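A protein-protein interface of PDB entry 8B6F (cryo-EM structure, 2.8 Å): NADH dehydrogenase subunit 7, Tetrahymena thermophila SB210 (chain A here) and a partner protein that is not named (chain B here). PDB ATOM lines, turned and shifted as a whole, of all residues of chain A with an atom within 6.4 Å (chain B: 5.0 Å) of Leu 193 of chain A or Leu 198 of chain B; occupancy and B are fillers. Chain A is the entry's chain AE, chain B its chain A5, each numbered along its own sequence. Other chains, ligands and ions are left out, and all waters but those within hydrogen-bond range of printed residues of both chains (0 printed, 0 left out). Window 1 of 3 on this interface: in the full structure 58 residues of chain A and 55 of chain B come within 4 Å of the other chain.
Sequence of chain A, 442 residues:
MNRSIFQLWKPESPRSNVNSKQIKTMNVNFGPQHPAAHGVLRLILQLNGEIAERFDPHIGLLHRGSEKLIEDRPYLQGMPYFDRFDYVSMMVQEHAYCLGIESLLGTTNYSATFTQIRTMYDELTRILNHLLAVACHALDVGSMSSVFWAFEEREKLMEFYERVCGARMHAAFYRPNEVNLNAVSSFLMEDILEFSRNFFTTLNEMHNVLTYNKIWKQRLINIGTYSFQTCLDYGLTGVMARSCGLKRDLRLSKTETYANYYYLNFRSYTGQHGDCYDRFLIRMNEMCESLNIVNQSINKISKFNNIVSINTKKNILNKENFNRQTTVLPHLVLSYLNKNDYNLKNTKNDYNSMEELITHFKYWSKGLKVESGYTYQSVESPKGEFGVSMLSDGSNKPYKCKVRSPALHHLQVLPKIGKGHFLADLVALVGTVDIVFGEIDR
Printed residues of chain B within 4 Å of Ser 196 of chain A: Leu 198 (3.95 Å). Of the printed residues of chain A, Lys 195 of chain B touches Phe 200. Printed residues of chain A within 4 Å of Glu 199 of chain B: Arg 197. Of the printed residues of chain B, Phe 200 of chain A touches Val 194 (3.8 Å), Lys 195 (3.4 Å) and Leu 198 (3.9 Å). The nearest residue of chain A that does not touch Leu 198 of chain B is Asn 295 of chain A (4.5 Å).
Of the 20 printed residues of chain A, 5 touch a printed residue of chain B. Of the 10 printed residues of chain B, 5 touch a printed residue of chain A. Printed residues of chain B that touch a printed residue of chain A: Val 194, Lys 195, Leu 198, Glu 199 and Phe 202. Along chain B the printed residues that touch a printed residue of chain A span positions 194 to 202. Among the printed residues, Asp or Glu carboxylates within 4 Å of a Lys or Arg side-chain nitrogen of the other chain: Arg 197 of chain A with Glu 199 of chain B (2.8 Å).
The backbone carbonyl oxygen of Glu 194 of chain A lies close to the side-chain amide oxygen of Asn 198 of chain A (3.4 Å). The side-chain hydroxyl of Ser 196 of chain A sits at hydrogen-bond distance from the backbone carbonyl oxygen of Ile 192 of chain A (2.9 Å).
NH2 of Arg 197 of chain A is in salt-bridge range of OE2 of Glu 199 of chain B, 2.8 Å away.
Among the printed residues, pairs that only touch across the chains: Leu 193 of chain A with Phe 202 of chain B (3.2 Å), Phe 200 of chain A with Lys 195 of chain B (3.4 Å), Arg 197 of chain A with Phe 202 of chain B (3.4 Å), Glu 194 of chain A with Phe 202 of chain B (3.5 Å), Arg 197 of chain A with Leu 198 of chain B (3.6 Å), Phe 200 of chain A with Val 194 of chain B (3.8 Å), Leu 193 of chain A with Leu 198 of chain B (3.9 Å), Phe 200 of chain A with Leu 198 of chain B (3.9 Å) and Ser 196 of chain A with Leu 198 of chain B (3.95 Å).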
ATOM      1  N   PHE A 160     -28.203 -16.218  -9.519  1.00  0.00           N
ATOM      2  CA  PHE A 160     -27.035 -16.124 -10.389  1.00  0.00           C
ATOM      3  C   PHE A 160     -26.360 -14.764 -10.244  1.00  0.00           C
ATOM      4  O   PHE A 160     -25.129 -14.678 -10.184  1.00  0.00           O
ATOM      5  CB  PHE A 160     -27.438 -16.361 -11.848  1.00  0.00           C
ATOM      6  CG  PHE A 160     -27.870 -17.774 -12.148  1.00  0.00           C
ATOM      7  CD1 PHE A 160     -27.361 -18.850 -11.438  1.00  0.00           C
ATOM      8  CD2 PHE A 160     -28.788 -18.022 -13.155  1.00  0.00           C
ATOM      9  CE1 PHE A 160     -27.763 -20.138 -11.723  1.00  0.00           C
ATOM     10  CE2 PHE A 160     -29.193 -19.308 -13.443  1.00  0.00           C
ATOM     11  CZ  PHE A 160     -28.680 -20.368 -12.726  1.00  0.00           C
ATOM     12  N   LEU A 188     -20.785 -21.859 -12.170  1.00  0.00           N
ATOM     13  CA  LEU A 188     -21.829 -20.881 -12.444  1.00  0.00           C
ATOM     14  C   LEU A 188     -22.400 -21.081 -13.840  1.00  0.00           C
ATOM     15  O   LEU A 188     -23.619 -21.027 -14.034  1.00  0.00           O
ATOM     16  CB  LEU A 188     -21.263 -19.475 -12.285  1.00  0.00           C
ATOM     17  CG  LEU A 188     -22.209 -18.314 -12.568  1.00  0.00           C
ATOM     18  CD1 LEU A 188     -23.394 -18.318 -11.627  1.00  0.00           C
ATOM     19  CD2 LEU A 188     -21.421 -17.028 -12.448  1.00  0.00           C
ATOM     20  N   MET A 189     -21.535 -21.328 -14.824  1.00  0.00           N
ATOM     21  CA  MET A 189     -22.007 -21.580 -16.181  1.00  0.00           C
ATOM     22  C   MET A 189     -22.857 -22.844 -16.245  1.00  0.00           C
ATOM     23  O   MET A 189     -23.885 -22.876 -16.929  1.00  0.00           O
ATOM     24  CB  MET A 189     -20.818 -21.697 -17.132  1.00  0.00           C
ATOM     25  CG  MET A 189     -19.906 -20.487 -17.151  1.00  0.00           C
ATOM     26  SD  MET A 189     -20.724 -19.013 -17.774  1.00  0.00           S
ATOM     27  CE  MET A 189     -19.422 -17.802 -17.589  1.00  0.00           C
ATOM     28  N   GLU A 190     -22.442 -23.898 -15.540  1.00  0.00           N
ATOM     29  CA  GLU A 190     -23.218 -25.135 -15.534  1.00  0.00           C
ATOM     30  C   GLU A 190     -24.590 -24.922 -14.909  1.00  0.00           C
ATOM     31  O   GLU A 190     -25.596 -25.438 -15.410  1.00  0.00           O
ATOM     32  CB  GLU A 190     -22.456 -26.231 -14.792  1.00  0.00           C
ATOM     33  CG  GLU A 190     -21.124 -26.577 -15.430  1.00  0.00           C
ATOM     34  CD  GLU A 190     -20.372 -27.638 -14.659  1.00  0.00           C
ATOM     35  OE1 GLU A 190     -20.843 -28.030 -13.572  1.00  0.00           O
ATOM     36  OE2 GLU A 190     -19.309 -28.082 -15.142  1.00  0.00           O
ATOM     37  N   ASP A 191     -24.653 -24.166 -13.813  1.00  0.00           N
ATOM     38  CA  ASP A 191     -25.940 -23.868 -13.195  1.00  0.00           C
ATOM     39  C   ASP A 191     -26.811 -23.031 -14.122  1.00  0.00           C
ATOM     40  O   ASP A 191     -28.031 -23.217 -14.177  1.00  0.00           O
ATOM     41  CB  ASP A 191     -25.730 -23.155 -11.862  1.00  0.00           C
ATOM     42  CG  ASP A 191     -25.268 -24.096 -10.767  1.00  0.00           C
ATOM     43  OD1 ASP A 191     -24.182 -24.694 -10.911  1.00  0.00           O
ATOM     44  OD2 ASP A 191     -25.991 -24.235  -9.760  1.00  0.00           O
ATOM     45  N   ILE A 192     -26.201 -22.103 -14.860  1.00  0.00           N
ATOM     46  CA  ILE A 192     -26.956 -21.319 -15.833  1.00  0.00           C
ATOM     47  C   ILE A 192     -27.517 -22.227 -16.919  1.00  0.00           C
ATOM     48  O   ILE A 192     -28.652 -22.045 -17.375  1.00  0.00           O
ATOM     49  CB  ILE A 192     -26.075 -20.200 -16.418  1.00  0.00           C
ATOM     50  CG1 ILE A 192     -25.793 -19.148 -15.344  1.00  0.00           C
ATOM     51  CG2 ILE A 192     -26.748 -19.552 -17.622  1.00  0.00           C
ATOM     52  CD1 ILE A 192     -24.735 -18.144 -15.722  1.00  0.00           C
ATOM     53  N   LEU A 193     -26.737 -23.220 -17.349  1.00  0.00           N
ATOM     54  CA  LEU A 193     -27.236 -24.168 -18.339  1.00  0.00           C
ATOM     55  C   LEU A 193     -28.420 -24.959 -17.795  1.00  0.00           C
ATOM     56  O   LEU A 193     -29.405 -25.180 -18.506  1.00  0.00           O
ATOM     57  CB  LEU A 193     -26.117 -25.113 -18.772  1.00  0.00           C
ATOM     58  CG  LEU A 193     -24.975 -24.487 -19.574  1.00  0.00           C
ATOM     59  CD1 LEU A 193     -23.860 -25.495 -19.770  1.00  0.00           C
ATOM     60  CD2 LEU A 193     -25.462 -23.966 -20.916  1.00  0.00           C
ATOM     61  N   GLU A 194     -28.337 -25.402 -16.540  1.00  0.00           N
ATOM     62  CA  GLU A 194     -29.460 -26.108 -15.933  1.00  0.00           C
ATOM     63  C   GLU A 194     -30.691 -25.217 -15.862  1.00  0.00           C
ATOM     64  O   GLU A 194     -31.808 -25.662 -16.148  1.00  0.00           O
ATOM     65  CB  GLU A 194     -29.087 -26.605 -14.542  1.00  0.00           C
ATOM     66  CG  GLU A 194     -30.210 -27.364 -13.866  1.00  0.00           C
ATOM     67  CD  GLU A 194     -29.853 -27.765 -12.464  1.00  0.00           C
ATOM     68  OE1 GLU A 194     -28.692 -27.531 -12.069  1.00  0.00           O
ATOM     69  OE2 GLU A 194     -30.730 -28.304 -11.756  1.00  0.00           O
ATOM     70  N   PHE A 195     -30.510 -23.955 -15.472  1.00  0.00           N
ATOM     71  CA  PHE A 195     -31.629 -23.022 -15.454  1.00  0.00           C
ATOM     72  C   PHE A 195     -32.227 -22.871 -16.843  1.00  0.00           C
ATOM     73  O   PHE A 195     -33.452 -22.840 -17.003  1.00  0.00           O
ATOM     74  CB  PHE A 195     -31.179 -21.660 -14.929  1.00  0.00           C
ATOM     75  CG  PHE A 195     -32.102 -20.543 -15.314  1.00  0.00           C
ATOM     76  CD1 PHE A 195     -33.194 -20.229 -14.526  1.00  0.00           C
ATOM     77  CD2 PHE A 195     -31.885 -19.818 -16.474  1.00  0.00           C
ATOM     78  CE1 PHE A 195     -34.050 -19.210 -14.886  1.00  0.00           C
ATOM     79  CE2 PHE A 195     -32.738 -18.801 -16.839  1.00  0.00           C
ATOM     80  CZ  PHE A 195     -33.822 -18.494 -16.043  1.00  0.00           C
ATOM     81  N   SER A 196     -31.374 -22.786 -17.865  1.00  0.00           N
ATOM     82  CA  SER A 196     -31.869 -22.666 -19.230  1.00  0.00           C
ATOM     83  C   SER A 196     -32.698 -23.881 -19.619  1.00  0.00           C
ATOM     84  O   SER A 196     -33.753 -23.745 -20.249  1.00  0.00           O
ATOM     85  CB  SER A 196     -30.698 -22.490 -20.197  1.00  0.00           C
ATOM     86  OG  SER A 196     -29.955 -21.324 -19.892  1.00  0.00           O
ATOM     87  N   ARG A 197     -32.243 -25.081 -19.257  1.00  0.00           N
ATOM     88  CA  ARG A 197     -33.013 -26.275 -19.585  1.00  0.00           C
ATOM     89  C   ARG A 197     -34.372 -26.262 -18.899  1.00  0.00           C
ATOM     90  O   ARG A 197     -35.385 -26.615 -19.512  1.00  0.00           O
ATOM     91  CB  ARG A 197     -32.229 -27.529 -19.197  1.00  0.00           C
ATOM     92  CG  ARG A 197     -33.004 -28.828 -19.382  1.00  0.00           C
ATOM     93  CD  ARG A 197     -33.478 -29.001 -20.816  1.00  0.00           C
ATOM     94  NE  ARG A 197     -34.323 -30.177 -20.983  1.00  0.00           N
ATOM     95  CZ  ARG A 197     -35.645 -30.179 -20.882  1.00  0.00           C
ATOM     96  NH1 ARG A 197     -36.321 -29.079 -20.596  1.00  0.00           N
ATOM     97  NH2 ARG A 197     -36.309 -31.313 -21.080  1.00  0.00           N
ATOM     98  N   ASN A 198     -34.416 -25.864 -17.629  1.00  0.00           N
ATOM     99  CA  ASN A 198     -35.671 -25.880 -16.890  1.00  0.00           C
ATOM    100  C   ASN A 198     -36.568 -24.696 -17.222  1.00  0.00           C
ATOM    101  O   ASN A 198     -37.756 -24.728 -16.889  1.00  0.00           O
ATOM    102  CB  ASN A 198     -35.399 -25.903 -15.386  1.00  0.00           C
ATOM    103  CG  ASN A 198     -35.104 -27.295 -14.869  1.00  0.00           C
ATOM    104  OD1 ASN A 198     -34.022 -27.561 -14.349  1.00  0.00           O
ATOM    105  ND2 ASN A 198     -36.072 -28.195 -15.010  1.00  0.00           N
ATOM    106  N   PHE A 200     -37.679 -23.785 -20.075  1.00  0.00           N
ATOM    107  CA  PHE A 200     -38.698 -24.163 -21.046  1.00  0.00           C
ATOM    108  C   PHE A 200     -39.980 -24.599 -20.353  1.00  0.00           C
ATOM    109  O   PHE A 200     -41.083 -24.325 -20.837  1.00  0.00           O
ATOM    110  CB  PHE A 200     -38.176 -25.278 -21.950  1.00  0.00           C
ATOM    111  CG  PHE A 200     -37.045 -24.857 -22.838  1.00  0.00           C
ATOM    112  CD1 PHE A 200     -37.291 -24.139 -23.996  1.00  0.00           C
ATOM    113  CD2 PHE A 200     -35.740 -25.187 -22.522  1.00  0.00           C
ATOM    114  CE1 PHE A 200     -36.252 -23.752 -24.820  1.00  0.00           C
ATOM    115  CE2 PHE A 200     -34.695 -24.803 -23.342  1.00  0.00           C
ATOM    116  CZ  PHE A 200     -34.952 -24.084 -24.491  1.00  0.00           C
ATOM    117  N   LEU A 291     -32.478 -18.055 -24.274  1.00  0.00           N
ATOM    118  CA  LEU A 291     -31.874 -19.335 -23.922  1.00  0.00           C
ATOM    119  C   LEU A 291     -30.904 -19.797 -24.997  1.00  0.00           C
ATOM    120  O   LEU A 291     -29.801 -20.262 -24.692  1.00  0.00           O
ATOM    121  CB  LEU A 291     -32.956 -20.392 -23.706  1.00  0.00           C
ATOM    122  CG  LEU A 291     -33.964 -20.166 -22.580  1.00  0.00           C
ATOM    123  CD1 LEU A 291     -34.896 -21.360 -22.494  1.00  0.00           C
ATOM    124  CD2 LEU A 291     -33.267 -19.923 -21.256  1.00  0.00           C
ATOM    125  N   VAL A 294     -27.777 -17.633 -24.839  1.00  0.00           N
ATOM    126  CA  VAL A 294     -26.943 -18.006 -23.700  1.00  0.00           C
ATOM    127  C   VAL A 294     -26.217 -19.313 -23.982  1.00  0.00           C
ATOM    128  O   VAL A 294     -25.036 -19.469 -23.650  1.00  0.00           O
ATOM    129  CB  VAL A 294     -27.794 -18.090 -22.418  1.00  0.00           C
ATOM    130  CG1 VAL A 294     -27.011 -18.735 -21.281  1.00  0.00           C
ATOM    131  CG2 VAL A 294     -28.263 -16.708 -22.003  1.00  0.00           C
ATOM    132  N   ASN A 295     -26.909 -20.273 -24.593  1.00  0.00           N
ATOM    133  CA  ASN A 295     -26.271 -21.542 -24.922  1.00  0.00           C
ATOM    134  C   ASN A 295     -25.106 -21.330 -25.881  1.00  0.00           C
ATOM    135  O   ASN A 295     -24.022 -21.894 -25.693  1.00  0.00           O
ATOM    136  CB  ASN A 295     -27.297 -22.500 -25.523  1.00  0.00           C
ATOM    137  CG  ASN A 295     -26.685 -23.819 -25.937  1.00  0.00           C
ATOM    138  OD1 ASN A 295     -25.681 -24.252 -25.377  1.00  0.00           O
ATOM    139  ND2 ASN A 295     -27.287 -24.464 -26.927  1.00  0.00           N
ATOM    140  N   ILE A 298     -22.162 -19.676 -23.990  1.00  0.00           N
ATOM    141  CA  ILE A 298     -21.448 -20.606 -23.121  1.00  0.00           C
ATOM    142  C   ILE A 298     -20.643 -21.598 -23.950  1.00  0.00           C
ATOM    143  O   ILE A 298     -19.537 -21.993 -23.565  1.00  0.00           O
ATOM    144  CB  ILE A 298     -22.430 -21.312 -22.168  1.00  0.00           C
ATOM    145  CG1 ILE A 298     -23.033 -20.292 -21.199  1.00  0.00           C
ATOM    146  CG2 ILE A 298     -21.725 -22.425 -21.396  1.00  0.00           C
ATOM    147  CD1 ILE A 298     -24.159 -20.834 -20.341  1.00  0.00           C
ATOM    148  N   ASN A 299     -21.183 -22.026 -25.093  1.00  0.00           N
ATOM    149  CA  ASN A 299     -20.434 -22.928 -25.960  1.00  0.00           C
ATOM    150  C   ASN A 299     -19.184 -22.262 -26.520  1.00  0.00           C
ATOM    151  O   ASN A 299     -18.193 -22.943 -26.801  1.00  0.00           O
ATOM    152  CB  ASN A 299     -21.320 -23.418 -27.103  1.00  0.00           C
ATOM    153  CG  ASN A 299     -22.499 -24.230 -26.617  1.00  0.00           C
ATOM    154  OD1 ASN A 299     -22.498 -24.737 -25.497  1.00  0.00           O
ATOM    155  ND2 ASN A 299     -23.510 -24.370 -27.466  1.00  0.00           N
ATOM    156  N   THR A 327     -16.716 -28.949 -18.714  1.00  0.00           N
ATOM    157  CA  THR A 327     -16.401 -28.733 -20.119  1.00  0.00           C
ATOM    158  C   THR A 327     -16.399 -27.260 -20.508  1.00  0.00           C
ATOM    159  O   THR A 327     -16.061 -26.942 -21.652  1.00  0.00           O
ATOM    160  CB  THR A 327     -17.395 -29.487 -21.009  1.00  0.00           C
ATOM    161  OG1 THR A 327     -18.722 -28.998 -20.775  1.00  0.00           O
ATOM    162  CG2 THR A 327     -17.351 -30.979 -20.717  1.00  0.00           C
ATOM    163  N   VAL A 328     -16.765 -26.358 -19.601  1.00  0.00           N
ATOM    164  CA  VAL A 328     -16.804 -24.925 -19.877  1.00  0.00           C
ATOM    165  C   VAL A 328     -15.678 -24.256 -19.101  1.00  0.00           C
ATOM    166  O   VAL A 328     -15.557 -24.437 -17.884  1.00  0.00           O
ATOM    167  CB  VAL A 328     -18.175 -24.314 -19.526  1.00  0.00           C
ATOM    168  CG1 VAL A 328     -19.285 -25.022 -20.280  1.00  0.00           C
ATOM    169  CG2 VAL A 328     -18.441 -24.375 -18.041  1.00  0.00           C
ATOM    170  N   GLN B 193     -33.513 -28.688 -30.610  1.00  0.00           N
ATOM    171  CA  GLN B 193     -32.086 -28.977 -30.561  1.00  0.00           C
ATOM    172  C   GLN B 193     -31.420 -28.315 -29.363  1.00  0.00           C
ATOM    173  O   GLN B 193     -30.468 -28.870 -28.805  1.00  0.00           O
ATOM    174  CB  GLN B 193     -31.416 -28.527 -31.858  1.00  0.00           C
ATOM    175  CG  GLN B 193     -29.998 -29.040 -32.023  1.00  0.00           C
ATOM    176  CD  GLN B 193     -29.932 -30.552 -32.078  1.00  0.00           C
ATOM    177  OE1 GLN B 193     -30.808 -31.202 -32.643  1.00  0.00           O
ATOM    178  NE2 GLN B 193     -28.893 -31.120 -31.480  1.00  0.00           N
ATOM    179  N   VAL B 194     -31.896 -27.139 -28.953  1.00  0.00           N
ATOM    180  CA  VAL B 194     -31.350 -26.499 -27.758  1.00  0.00           C
ATOM    181  C   VAL B 194     -31.613 -27.369 -26.534  1.00  0.00           C
ATOM    182  O   VAL B 194     -30.719 -27.600 -25.713  1.00  0.00           O
ATOM    183  CB  VAL B 194     -31.937 -25.085 -27.586  1.00  0.00           C
ATOM    184  CG1 VAL B 194     -31.560 -24.501 -26.230  1.00  0.00           C
ATOM    185  CG2 VAL B 194     -31.458 -24.171 -28.697  1.00  0.00           C
ATOM    186  N   LYS B 195     -32.842 -27.864 -26.394  1.00  0.00           N
ATOM    187  CA  LYS B 195     -33.150 -28.759 -25.284  1.00  0.00           C
ATOM    188  C   LYS B 195     -32.253 -29.988 -25.314  1.00  0.00           C
ATOM    189  O   LYS B 195     -31.695 -30.392 -24.288  1.00  0.00           O
ATOM    190  CB  LYS B 195     -34.619 -29.179 -25.343  1.00  0.00           C
ATOM    191  CG  LYS B 195     -35.607 -28.110 -24.932  1.00  0.00           C
ATOM    192  CD  LYS B 195     -37.026 -28.652 -24.999  1.00  0.00           C
ATOM    193  CE  LYS B 195     -38.018 -27.697 -24.368  1.00  0.00           C
ATOM    194  NZ  LYS B 195     -39.409 -28.220 -24.439  1.00  0.00           N
ATOM    195  N   LEU B 196     -32.111 -30.603 -26.488  1.00  0.00           N
ATOM    196  CA  LEU B 196     -31.302 -31.811 -26.601  1.00  0.00           C
ATOM    197  C   LEU B 196     -29.842 -31.533 -26.265  1.00  0.00           C
ATOM    198  O   LEU B 196     -29.188 -32.339 -25.594  1.00  0.00           O
ATOM    199  CB  LEU B 196     -31.430 -32.393 -28.007  1.00  0.00           C
ATOM    200  CG  LEU B 196     -32.818 -32.926 -28.373  1.00  0.00           C
ATOM    201  CD1 LEU B 196     -32.843 -33.389 -29.813  1.00  0.00           C
ATOM    202  CD2 LEU B 196     -33.260 -34.043 -27.440  1.00  0.00           C
ATOM    203  N   ASP B 197     -29.313 -30.398 -26.725  1.00  0.00           N
ATOM    204  CA  ASP B 197     -27.927 -30.057 -26.422  1.00  0.00           C
ATOM    205  C   ASP B 197     -27.728 -29.835 -24.931  1.00  0.00           C
ATOM    206  O   ASP B 197     -26.712 -30.255 -24.366  1.00  0.00           O
ATOM    207  CB  ASP B 197     -27.507 -28.810 -27.200  1.00  0.00           C
ATOM    208  CG  ASP B 197     -27.437 -29.049 -28.694  1.00  0.00           C
ATOM    209  OD1 ASP B 197     -27.723 -30.181 -29.133  1.00  0.00           O
ATOM    210  OD2 ASP B 197     -27.091 -28.103 -29.430  1.00  0.00           O
ATOM    211  N   LEU B 198     -28.679 -29.169 -24.276  1.00  0.00           N
ATOM    212  CA  LEU B 198     -28.568 -28.963 -22.836  1.00  0.00           C
ATOM    213  C   LEU B 198     -28.548 -30.293 -22.097  1.00  0.00           C
ATOM    214  O   LEU B 198     -27.710 -30.515 -21.217  1.00  0.00           O
ATOM    215  CB  LEU B 198     -29.722 -28.089 -22.348  1.00  0.00           C
ATOM    216  CG  LEU B 198     -29.715 -26.648 -22.863  1.00  0.00           C
ATOM    217  CD1 LEU B 198     -31.023 -25.959 -22.533  1.00  0.00           C
ATOM    218  CD2 LEU B 198     -28.547 -25.873 -22.283  1.00  0.00           C
ATOM    219  N   GLU B 199     -29.464 -31.198 -22.445  1.00  0.00           N
ATOM    220  CA  GLU B 199     -29.497 -32.499 -21.783  1.00  0.00           C
ATOM    221  C   GLU B 199     -28.232 -33.292 -22.083  1.00  0.00           C
ATOM    222  O   GLU B 199     -27.719 -34.009 -21.219  1.00  0.00           O
ATOM    223  CB  GLU B 199     -30.741 -33.274 -22.207  1.00  0.00           C
ATOM    224  CG  GLU B 199     -32.036 -32.587 -21.814  1.00  0.00           C
ATOM    225  CD  GLU B 199     -33.255 -33.454 -22.041  1.00  0.00           C
ATOM    226  OE1 GLU B 199     -33.120 -34.693 -22.011  1.00  0.00           O
ATOM    227  OE2 GLU B 199     -34.350 -32.892 -22.248  1.00  0.00           O
ATOM    228  N   TRP B 200     -27.723 -33.182 -23.311  1.00  0.00           N
ATOM    229  CA  TRP B 200     -26.483 -33.865 -23.666  1.00  0.00           C
ATOM    230  C   TRP B 200     -25.317 -33.346 -22.833  1.00  0.00           C
ATOM    231  O   TRP B 200     -24.485 -34.129 -22.362  1.00  0.00           O
ATOM    232  CB  TRP B 200     -26.205 -33.689 -25.159  1.00  0.00           C
ATOM    233  CG  TRP B 200     -24.924 -34.314 -25.628  1.00  0.00           C
ATOM    234  CD1 TRP B 200     -24.744 -35.600 -26.042  1.00  0.00           C
ATOM    235  CD2 TRP B 200     -23.646 -33.673 -25.742  1.00  0.00           C
ATOM    236  NE1 TRP B 200     -23.434 -35.803 -26.402  1.00  0.00           N
ATOM    237  CE2 TRP B 200     -22.740 -34.635 -26.227  1.00  0.00           C
ATOM    238  CE3 TRP B 200     -23.182 -32.381 -25.477  1.00  0.00           C
ATOM    239  CZ2 TRP B 200     -21.396 -34.347 -26.453  1.00  0.00           C
ATOM    240  CZ3 TRP B 200     -21.847 -32.096 -25.702  1.00  0.00           C
ATOM    241  CH2 TRP B 200     -20.969 -33.075 -26.185  1.00  0.00           C
ATOM    242  N   THR B 201     -25.238 -32.028 -22.645  1.00  0.00           N
ATOM    243  CA  THR B 201     -24.175 -31.465 -21.818  1.00  0.00           C
ATOM    244  C   THR B 201     -24.283 -31.950 -20.377  1.00  0.00           C
ATOM    245  O   THR B 201     -23.273 -32.299 -19.756  1.00  0.00           O
ATOM    246  CB  THR B 201     -24.224 -29.938 -21.868  1.00  0.00           C
ATOM    247  OG1 THR B 201     -24.049 -29.493 -23.219  1.00  0.00           O
ATOM    248  CG2 THR B 201     -23.130 -29.331 -20.997  1.00  0.00           C
ATOM    249  N   PHE B 202     -25.497 -31.973 -19.825  1.00  0.00           N
ATOM    250  CA  PHE B 202     -25.668 -32.454 -18.458  1.00  0.00           C
ATOM    251  C   PHE B 202     -25.239 -33.908 -18.333  1.00  0.00           C
ATOM    252  O   PHE B 202     -24.563 -34.284 -17.369  1.00  0.00           O
ATOM    253  CB  PHE B 202     -27.122 -32.290 -18.019  1.00  0.00           C
ATOM    254  CG  PHE B 202     -27.644 -30.892 -18.170  1.00  0.00           C
ATOM    255  CD1 PHE B 202     -26.806 -29.800 -18.003  1.00  0.00           C
ATOM    256  CD2 PHE B 202     -28.969 -30.670 -18.495  1.00  0.00           C
ATOM    257  CE1 PHE B 202     -27.285 -28.517 -18.147  1.00  0.00           C
ATOM    258  CE2 PHE B 202     -29.453 -29.389 -18.641  1.00  0.00           C
ATOM    259  CZ  PHE B 202     -28.610 -28.311 -18.469  1.00  0.00           C
